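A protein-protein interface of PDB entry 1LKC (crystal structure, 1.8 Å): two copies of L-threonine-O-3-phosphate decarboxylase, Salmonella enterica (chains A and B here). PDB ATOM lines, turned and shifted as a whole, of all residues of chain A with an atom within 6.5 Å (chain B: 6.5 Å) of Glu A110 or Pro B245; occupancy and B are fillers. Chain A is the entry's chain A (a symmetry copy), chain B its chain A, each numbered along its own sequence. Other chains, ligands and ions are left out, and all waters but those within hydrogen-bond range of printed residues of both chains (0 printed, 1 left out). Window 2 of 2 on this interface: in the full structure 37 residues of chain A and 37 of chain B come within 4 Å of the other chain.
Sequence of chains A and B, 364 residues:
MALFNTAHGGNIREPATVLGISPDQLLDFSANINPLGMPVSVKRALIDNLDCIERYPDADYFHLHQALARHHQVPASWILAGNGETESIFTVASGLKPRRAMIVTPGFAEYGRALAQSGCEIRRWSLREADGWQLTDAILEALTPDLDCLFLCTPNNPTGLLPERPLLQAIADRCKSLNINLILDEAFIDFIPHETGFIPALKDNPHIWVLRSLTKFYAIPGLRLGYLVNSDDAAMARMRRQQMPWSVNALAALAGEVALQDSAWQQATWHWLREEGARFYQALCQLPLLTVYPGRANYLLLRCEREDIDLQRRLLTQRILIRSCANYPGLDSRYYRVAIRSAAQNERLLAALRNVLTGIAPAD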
ATOM      1  N   HIS A   8      11.597  13.185  27.356  1.00  0.00           N
ATOM      2  CA  HIS A   8      12.676  12.522  26.547  1.00  0.00           C
ATOM      3  C   HIS A   8      13.694  11.873  27.469  1.00  0.00           C
ATOM      4  O   HIS A   8      13.761  12.213  28.650  1.00  0.00           O
ATOM      5  CB  HIS A   8      13.417  13.547  25.672  1.00  0.00           C
ATOM      6  CG  HIS A   8      12.596  14.093  24.543  1.00  0.00           C
ATOM      7  ND1 HIS A   8      12.198  13.324  23.470  1.00  0.00           N
ATOM      8  CD2 HIS A   8      12.108  15.339  24.315  1.00  0.00           C
ATOM      9  CE1 HIS A   8      11.502  14.070  22.627  1.00  0.00           C
ATOM     10  NE2 HIS A   8      11.433  15.299  23.117  1.00  0.00           N
ATOM     11  N   ASN A  83      20.419  24.393  15.870  1.00  0.00           N
ATOM     12  CA  ASN A  83      20.792  24.295  17.292  1.00  0.00           C
ATOM     13  C   ASN A  83      20.199  22.932  17.708  1.00  0.00           C
ATOM     14  O   ASN A  83      19.173  22.872  18.427  1.00  0.00           O
ATOM     15  CB  ASN A  83      20.115  25.455  18.037  1.00  0.00           C
ATOM     16  CG  ASN A  83      20.426  25.506  19.512  1.00  0.00           C
ATOM     17  OD1 ASN A  83      19.541  25.833  20.356  1.00  0.00           O
ATOM     18  ND2 ASN A  83      21.658  25.251  19.850  1.00  0.00           N
ATOM     19  N   THR A  86      16.877  19.010  16.619  1.00  0.00           N
ATOM     20  CA  THR A  86      15.589  19.411  17.180  1.00  0.00           C
ATOM     21  C   THR A  86      15.196  20.758  16.543  1.00  0.00           C
ATOM     22  O   THR A  86      14.025  20.975  16.160  1.00  0.00           O
ATOM     23  CB  THR A  86      15.696  19.581  18.725  1.00  0.00           C
ATOM     24  OG1 THR A  86      15.837  18.277  19.325  1.00  0.00           O
ATOM     25  CG2 THR A  86      14.408  20.224  19.292  1.00  0.00           C
ATOM     26  N   GLU A  87      16.143  21.687  16.451  1.00  0.00           N
ATOM     27  CA  GLU A  87      15.788  22.963  15.823  1.00  0.00           C
ATOM     28  C   GLU A  87      15.421  22.742  14.373  1.00  0.00           C
ATOM     29  O   GLU A  87      14.441  23.319  13.885  1.00  0.00           O
ATOM     30  CB  GLU A  87      16.928  23.982  15.895  1.00  0.00           C
ATOM     31  CG  GLU A  87      16.487  25.295  15.296  1.00  0.00           C
ATOM     32  CD  GLU A  87      17.423  26.433  15.572  1.00  0.00           C
ATOM     33  OE1 GLU A  87      18.621  26.308  15.253  1.00  0.00           O
ATOM     34  OE2 GLU A  87      16.959  27.467  16.104  1.00  0.00           O
ATOM     35  N   ILE A  89      13.963  20.292  13.046  1.00  0.00           N
ATOM     36  CA  ILE A  89      12.573  19.748  12.984  1.00  0.00           C
ATOM     37  C   ILE A  89      11.584  20.927  13.072  1.00  0.00           C
ATOM     38  O   ILE A  89      10.614  20.988  12.308  1.00  0.00           O
ATOM     39  CB  ILE A  89      12.306  18.785  14.175  1.00  0.00           C
ATOM     40  CG1 ILE A  89      13.075  17.441  13.936  1.00  0.00           C
ATOM     41  CG2 ILE A  89      10.794  18.541  14.330  1.00  0.00           C
ATOM     42  CD1 ILE A  89      13.076  16.500  15.176  1.00  0.00           C
ATOM     43  N   PHE A  90      11.826  21.856  13.996  1.00  0.00           N
ATOM     44  CA  PHE A  90      10.908  23.002  14.103  1.00  0.00           C
ATOM     45  C   PHE A  90      11.029  23.913  12.923  1.00  0.00           C
ATOM     46  O   PHE A  90      10.032  24.510  12.481  1.00  0.00           O
ATOM     47  CB  PHE A  90      11.110  23.796  15.377  1.00  0.00           C
ATOM     48  CG  PHE A  90      10.510  23.115  16.573  1.00  0.00           C
ATOM     49  CD1 PHE A  90      11.182  22.044  17.178  1.00  0.00           C
ATOM     50  CD2 PHE A  90       9.250  23.499  17.051  1.00  0.00           C
ATOM     51  CE1 PHE A  90      10.616  21.359  18.241  1.00  0.00           C
ATOM     52  CE2 PHE A  90       8.668  22.823  18.123  1.00  0.00           C
ATOM     53  CZ  PHE A  90       9.331  21.757  18.722  1.00  0.00           C
ATOM     54  N   GLY A 107       6.700   6.817  17.387  1.00  0.00           N
ATOM     55  CA  GLY A 107       7.760   7.566  16.721  1.00  0.00           C
ATOM     56  C   GLY A 107       8.307   8.634  17.622  1.00  0.00           C
ATOM     57  O   GLY A 107       7.961   8.668  18.807  1.00  0.00           O
ATOM     58  N   PHE A 108       9.108   9.546  17.070  1.00  0.00           N
ATOM     59  CA  PHE A 108       9.715  10.629  17.834  1.00  0.00           C
ATOM     60  C   PHE A 108       8.663  11.751  18.104  1.00  0.00           C
ATOM     61  O   PHE A 108       8.116  12.313  17.182  1.00  0.00           O
ATOM     62  CB  PHE A 108      10.926  11.168  17.046  1.00  0.00           C
ATOM     63  CG  PHE A 108      11.805  12.074  17.835  1.00  0.00           C
ATOM     64  CD1 PHE A 108      12.462  11.608  18.975  1.00  0.00           C
ATOM     65  CD2 PHE A 108      11.968  13.430  17.465  1.00  0.00           C
ATOM     66  CE1 PHE A 108      13.266  12.469  19.750  1.00  0.00           C
ATOM     67  CE2 PHE A 108      12.761  14.287  18.231  1.00  0.00           C
ATOM     68  CZ  PHE A 108      13.411  13.808  19.379  1.00  0.00           C
ATOM     69  N   ALA A 109       8.418  12.071  19.374  1.00  0.00           N
ATOM     70  CA  ALA A 109       7.372  13.051  19.750  1.00  0.00           C
ATOM     71  C   ALA A 109       7.466  14.501  19.278  1.00  0.00           C
ATOM     72  O   ALA A 109       6.420  15.213  19.194  1.00  0.00           O
ATOM     73  CB  ALA A 109       7.228  13.042  21.253  1.00  0.00           C
ATOM     74  N   GLU A 110       8.680  14.972  19.017  1.00  0.00           N
ATOM     75  CA  GLU A 110       8.850  16.371  18.639  1.00  0.00           C
ATOM     76  C   GLU A 110       8.121  16.723  17.313  1.00  0.00           C
ATOM     77  O   GLU A 110       7.780  17.878  17.083  1.00  0.00           O
ATOM     78  CB  GLU A 110      10.355  16.747  18.557  1.00  0.00           C
ATOM     79  CG  GLU A 110      11.037  16.902  19.949  1.00  0.00           C
ATOM     80  CD  GLU A 110      10.208  17.715  20.979  1.00  0.00           C
ATOM     81  OE1 GLU A 110       9.733  18.817  20.669  1.00  0.00           O
ATOM     82  OE2 GLU A 110      10.045  17.266  22.138  1.00  0.00           O
ATOM     83  N   TYR A 111       7.871  15.747  16.438  1.00  0.00           N
ATOM     84  CA  TYR A 111       7.191  16.101  15.192  1.00  0.00           C
ATOM     85  C   TYR A 111       5.775  16.564  15.506  1.00  0.00           C
ATOM     86  O   TYR A 111       5.331  17.580  14.981  1.00  0.00           O
ATOM     87  CB  TYR A 111       7.127  14.909  14.213  1.00  0.00           C
ATOM     88  CG  TYR A 111       8.474  14.700  13.602  1.00  0.00           C
ATOM     89  CD1 TYR A 111       9.391  13.811  14.177  1.00  0.00           C
ATOM     90  CD2 TYR A 111       8.911  15.528  12.576  1.00  0.00           C
ATOM     91  CE1 TYR A 111      10.758  13.777  13.718  1.00  0.00           C
ATOM     92  CE2 TYR A 111      10.238  15.508  12.126  1.00  0.00           C
ATOM     93  CZ  TYR A 111      11.144  14.631  12.706  1.00  0.00           C
ATOM     94  OH  TYR A 111      12.442  14.635  12.251  1.00  0.00           O
ATOM     95  N   GLY A 112       5.075  15.786  16.322  1.00  0.00           N
ATOM     96  CA  GLY A 112       3.715  16.157  16.699  1.00  0.00           C
ATOM     97  C   GLY A 112       3.716  17.494  17.417  1.00  0.00           C
ATOM     98  O   GLY A 112       2.816  18.319  17.216  1.00  0.00           O
ATOM     99  N   ARG A 113       4.730  17.751  18.244  1.00  0.00           N
ATOM    100  CA  ARG A 113       4.739  19.040  18.947  1.00  0.00           C
ATOM    101  C   ARG A 113       4.969  20.188  18.009  1.00  0.00           C
ATOM    102  O   ARG A 113       4.289  21.220  18.105  1.00  0.00           O
ATOM    103  CB  ARG A 113       5.814  19.089  20.061  1.00  0.00           C
ATOM    104  CG  ARG A 113       5.635  18.035  21.141  1.00  0.00           C
ATOM    105  CD  ARG A 113       6.570  18.344  22.331  1.00  0.00           C
ATOM    106  NE  ARG A 113       6.250  19.616  22.997  1.00  0.00           N
ATOM    107  CZ  ARG A 113       6.990  20.734  22.963  1.00  0.00           C
ATOM    108  NH1 ARG A 113       8.137  20.800  22.297  1.00  0.00           N
ATOM    109  NH2 ARG A 113       6.564  21.817  23.605  1.00  0.00           N
ATOM    110  N   ALA A 114       5.928  20.037  17.093  1.00  0.00           N
ATOM    111  CA  ALA A 114       6.223  21.132  16.161  1.00  0.00           C
ATOM    112  C   ALA A 114       5.050  21.400  15.219  1.00  0.00           C
ATOM    113  O   ALA A 114       4.733  22.564  14.903  1.00  0.00           O
ATOM    114  CB  ALA A 114       7.512  20.798  15.340  1.00  0.00           C
ATOM    115  N   LEU A 115       4.393  20.339  14.778  1.00  0.00           N
ATOM    116  CA  LEU A 115       3.247  20.460  13.844  1.00  0.00           C
ATOM    117  C   LEU A 115       2.055  21.093  14.535  1.00  0.00           C
ATOM    118  O   LEU A 115       1.302  21.905  13.937  1.00  0.00           O
ATOM    119  CB  LEU A 115       2.835  19.074  13.319  1.00  0.00           C
ATOM    120  CG  LEU A 115       3.844  18.502  12.323  1.00  0.00           C
ATOM    121  CD1 LEU A 115       3.612  17.005  12.109  1.00  0.00           C
ATOM    122  CD2 LEU A 115       3.783  19.301  11.042  1.00  0.00           C
ATOM    123  N   ARG A 224      24.727  20.922  21.063  1.00  0.00           N
ATOM    124  CA  ARG A 224      23.571  21.113  20.165  1.00  0.00           C
ATOM    125  C   ARG A 224      23.879  21.404  18.699  1.00  0.00           C
ATOM    126  O   ARG A 224      24.017  22.568  18.302  1.00  0.00           O
ATOM    127  CB  ARG A 224      22.622  22.224  20.657  1.00  0.00           C
ATOM    128  CG  ARG A 224      22.395  22.270  22.192  1.00  0.00           C
ATOM    129  CD  ARG A 224      21.755  20.975  22.766  1.00  0.00           C
ATOM    130  NE  ARG A 224      20.494  20.699  22.091  1.00  0.00           N
ATOM    131  CZ  ARG A 224      20.201  19.591  21.421  1.00  0.00           C
ATOM    132  NH1 ARG A 224      21.072  18.583  21.329  1.00  0.00           N
ATOM    133  NH2 ARG A 224      19.033  19.512  20.768  1.00  0.00           N
ATOM    134  N   ALA B  59      17.220  19.342  30.692  1.00  0.00           N
ATOM    135  CA  ALA B  59      16.072  19.903  29.973  1.00  0.00           C
ATOM    136  C   ALA B  59      15.329  20.982  30.767  1.00  0.00           C
ATOM    137  O   ALA B  59      14.672  21.853  30.195  1.00  0.00           O
ATOM    138  CB  ALA B  59      15.098  18.782  29.589  1.00  0.00           C
ATOM    139  N   TYR B  61      17.003  22.925  33.144  1.00  0.00           N
ATOM    140  CA  TYR B  61      17.996  23.913  33.557  1.00  0.00           C
ATOM    141  C   TYR B  61      17.875  24.327  35.020  1.00  0.00           C
ATOM    142  O   TYR B  61      17.883  25.511  35.353  1.00  0.00           O
ATOM    143  CB  TYR B  61      17.934  25.146  32.619  1.00  0.00           C
ATOM    144  CG  TYR B  61      18.215  24.741  31.186  1.00  0.00           C
ATOM    145  CD1 TYR B  61      17.174  24.452  30.317  1.00  0.00           C
ATOM    146  CD2 TYR B  61      19.534  24.557  30.740  1.00  0.00           C
ATOM    147  CE1 TYR B  61      17.421  23.977  29.010  1.00  0.00           C
ATOM    148  CE2 TYR B  61      19.805  24.071  29.430  1.00  0.00           C
ATOM    149  CZ  TYR B  61      18.742  23.788  28.581  1.00  0.00           C
ATOM    150  OH  TYR B  61      18.969  23.324  27.292  1.00  0.00           O
ATOM    151  N   ARG B 241       6.602  25.793  27.697  1.00  0.00           N
ATOM    152  CA  ARG B 241       6.142  24.840  26.655  1.00  0.00           C
ATOM    153  C   ARG B 241       6.426  25.335  25.234  1.00  0.00           C
ATOM    154  O   ARG B 241       6.775  24.559  24.337  1.00  0.00           O
ATOM    155  CB  ARG B 241       4.627  24.587  26.805  1.00  0.00           C
ATOM    156  CG  ARG B 241       4.221  23.906  28.116  1.00  0.00           C
ATOM    157  CD  ARG B 241       2.759  23.392  28.051  1.00  0.00           C
ATOM    158  NE  ARG B 241       1.758  24.469  27.929  1.00  0.00           N
ATOM    159  CZ  ARG B 241       1.179  25.100  28.953  1.00  0.00           C
ATOM    160  NH1 ARG B 241       1.472  24.774  30.206  1.00  0.00           N
ATOM    161  NH2 ARG B 241       0.324  26.086  28.722  1.00  0.00           N
ATOM    162  N   GLN B 243       8.917  27.217  24.242  1.00  0.00           N
ATOM    163  CA  GLN B 243      10.334  27.182  23.923  1.00  0.00           C
ATOM    164  C   GLN B 243      10.804  25.780  23.536  1.00  0.00           C
ATOM    165  O   GLN B 243      10.397  24.773  24.098  1.00  0.00           O
ATOM    166  CB  GLN B 243      11.175  27.736  25.120  1.00  0.00           C
ATOM    167  N   MET B 244      11.681  25.715  22.552  1.00  0.00           N
ATOM    168  CA  MET B 244      12.177  24.422  22.088  1.00  0.00           C
ATOM    169  C   MET B 244      13.007  23.668  23.153  1.00  0.00           C
ATOM    170  O   MET B 244      13.750  24.264  23.915  1.00  0.00           O
ATOM    171  CB  MET B 244      13.001  24.701  20.846  1.00  0.00           C
ATOM    172  CG  MET B 244      13.509  23.515  20.145  1.00  0.00           C
ATOM    173  SD  MET B 244      14.430  24.211  18.740  1.00  0.00           S
ATOM    174  CE  MET B 244      16.201  24.228  19.491  1.00  0.00           C
ATOM    175  N   PRO B 245      12.889  22.342  23.213  1.00  0.00           N
ATOM    176  CA  PRO B 245      13.656  21.607  24.221  1.00  0.00           C
ATOM    177  C   PRO B 245      15.164  21.637  23.995  1.00  0.00           C
ATOM    178  O   PRO B 245      15.620  21.668  22.853  1.00  0.00           O
ATOM    179  CB  PRO B 245      13.080  20.195  24.142  1.00  0.00           C
ATOM    180  CG  PRO B 245      12.644  20.089  22.684  1.00  0.00           C
ATOM    181  CD  PRO B 245      12.045  21.441  22.408  1.00  0.00           C
ATOM    182  N   TRP B 246      15.900  21.660  25.101  1.00  0.00           N
ATOM    183  CA  TRP B 246      17.346  21.657  25.119  1.00  0.00           C
ATOM    184  C   TRP B 246      17.924  22.832  24.356  1.00  0.00           C
ATOM    185  O   TRP B 246      19.052  22.758  23.919  1.00  0.00           O
ATOM    186  CB  TRP B 246      17.876  20.387  24.467  1.00  0.00           C
ATOM    187  CG  TRP B 246      17.470  19.125  25.115  1.00  0.00           C
ATOM    188  CD1 TRP B 246      17.745  18.727  26.397  1.00  0.00           C
ATOM    189  CD2 TRP B 246      16.805  18.031  24.480  1.00  0.00           C
ATOM    190  NE1 TRP B 246      17.289  17.434  26.593  1.00  0.00           N
ATOM    191  CE2 TRP B 246      16.709  16.989  25.432  1.00  0.00           C
ATOM    192  CE3 TRP B 246      16.284  17.827  23.195  1.00  0.00           C
ATOM    193  CZ2 TRP B 246      16.109  15.759  25.138  1.00  0.00           C
ATOM    194  CZ3 TRP B 246      15.688  16.599  22.902  1.00  0.00           C
ATOM    195  CH2 TRP B 246      15.608  15.583  23.875  1.00  0.00           C
ATOM    196  N   SER B 247      17.212  23.940  24.235  1.00  0.00           N
ATOM    197  CA  SER B 247      17.740  24.995  23.401  1.00  0.00           C
ATOM    198  C   SER B 247      18.953  25.725  23.937  1.00  0.00           C
ATOM    199  O   SER B 247      19.657  26.341  23.143  1.00  0.00           O
ATOM    200  CB  SER B 247      16.650  26.041  23.099  1.00  0.00           C
ATOM    201  OG  SER B 247      16.401  26.762  24.281  1.00  0.00           O
ATOM    202  N   VAL B 248      19.177  25.691  25.253  1.00  0.00           N
ATOM    203  CA  VAL B 248      20.364  26.355  25.856  1.00  0.00           C
ATOM    204  C   VAL B 248      21.483  25.295  25.890  1.00  0.00           C
ATOM    205  O   VAL B 248      21.292  24.206  26.469  1.00  0.00           O
ATOM    206  CB  VAL B 248      19.990  26.865  27.240  1.00  0.00           C
ATOM    207  CG1 VAL B 248      21.241  27.315  28.054  1.00  0.00           C
ATOM    208  CG2 VAL B 248      19.025  28.057  27.047  1.00  0.00           C
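NH2 of Arg A113 is in hydrogen-bond range of O of Arg B241 (2.8 Å). The side-chain amide oxygen (OD1) of Asn A83 sits close to the backbone carbonyl oxygen (O) of Ser B247 (2.8 Å). The backbone carbonyl oxygen (O) of Trp B246 sits at hydrogen-bond distance from the guanidinium group (NE) of Arg A224.
His A8 touches Trp B246. Asn A83 touches Met B244. Thr A86 touches Met B244. Pro B245 touches Thr A86. Thr A86 touches Trp B246. Met B244 touches Glu A87. Glu A110 touches Pro B245. Pro B245 touches Arg A113 (CD to NH1, 3.96 Å).
Glu A110 touches just one residue of chain B: Pro B245 (3.8 Å). Of chain A, only Thr A86 (3.8 Å), Glu A110 (3.8 Å) and Arg A113 (3.96 Å) come within 4 Å of Pro B245. Of the printed residues of chain A, Trp B246 touches His A8, Thr A86 and Arg A224. Printed residues of chain B within 4 Å of Glu A87: Met B244. Gly A112 touches none of the printed residues of chain B. Gln B243 touches none of the printed residues of chain A. The nearest residue of chain A that does not touch Pro B245 is Phe A90 (4.4 Å). The nearest printed residue of chain B that does not touch Thr A86 is Ser B247 (6.8 Å).
No position is printed for both chains. Of the 11 pairs that touch across the chains among the printed residues, none has its exchanged pair printed and touching as well.
Hydrophobic or aromatic side chains of chain B within 4 Å of the printed part of chain A: Met B244, Pro B245 and Trp B246. Among the printed residues, 11 pairs touch across the chains.
The side-chain hydroxyl (OH) of Tyr B61 sits close to the backbone carbonyl oxygen (O) of Trp B246. A ring nitrogen (NE2) of His A8 lies within hydrogen-bond range of the side-chain carboxylate (OE2) of Glu A110. The side-chain carboxylate (OE1) of Glu A110 lies within salt-bridge range of the guanidinium group (NH1) of Arg A113, at 3.0 Å. The backbone NH (N) of Asn A83 lies within hydrogen-bond range of the side-chain carboxylate (OE1) of Glu A87 (2.7 Å).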
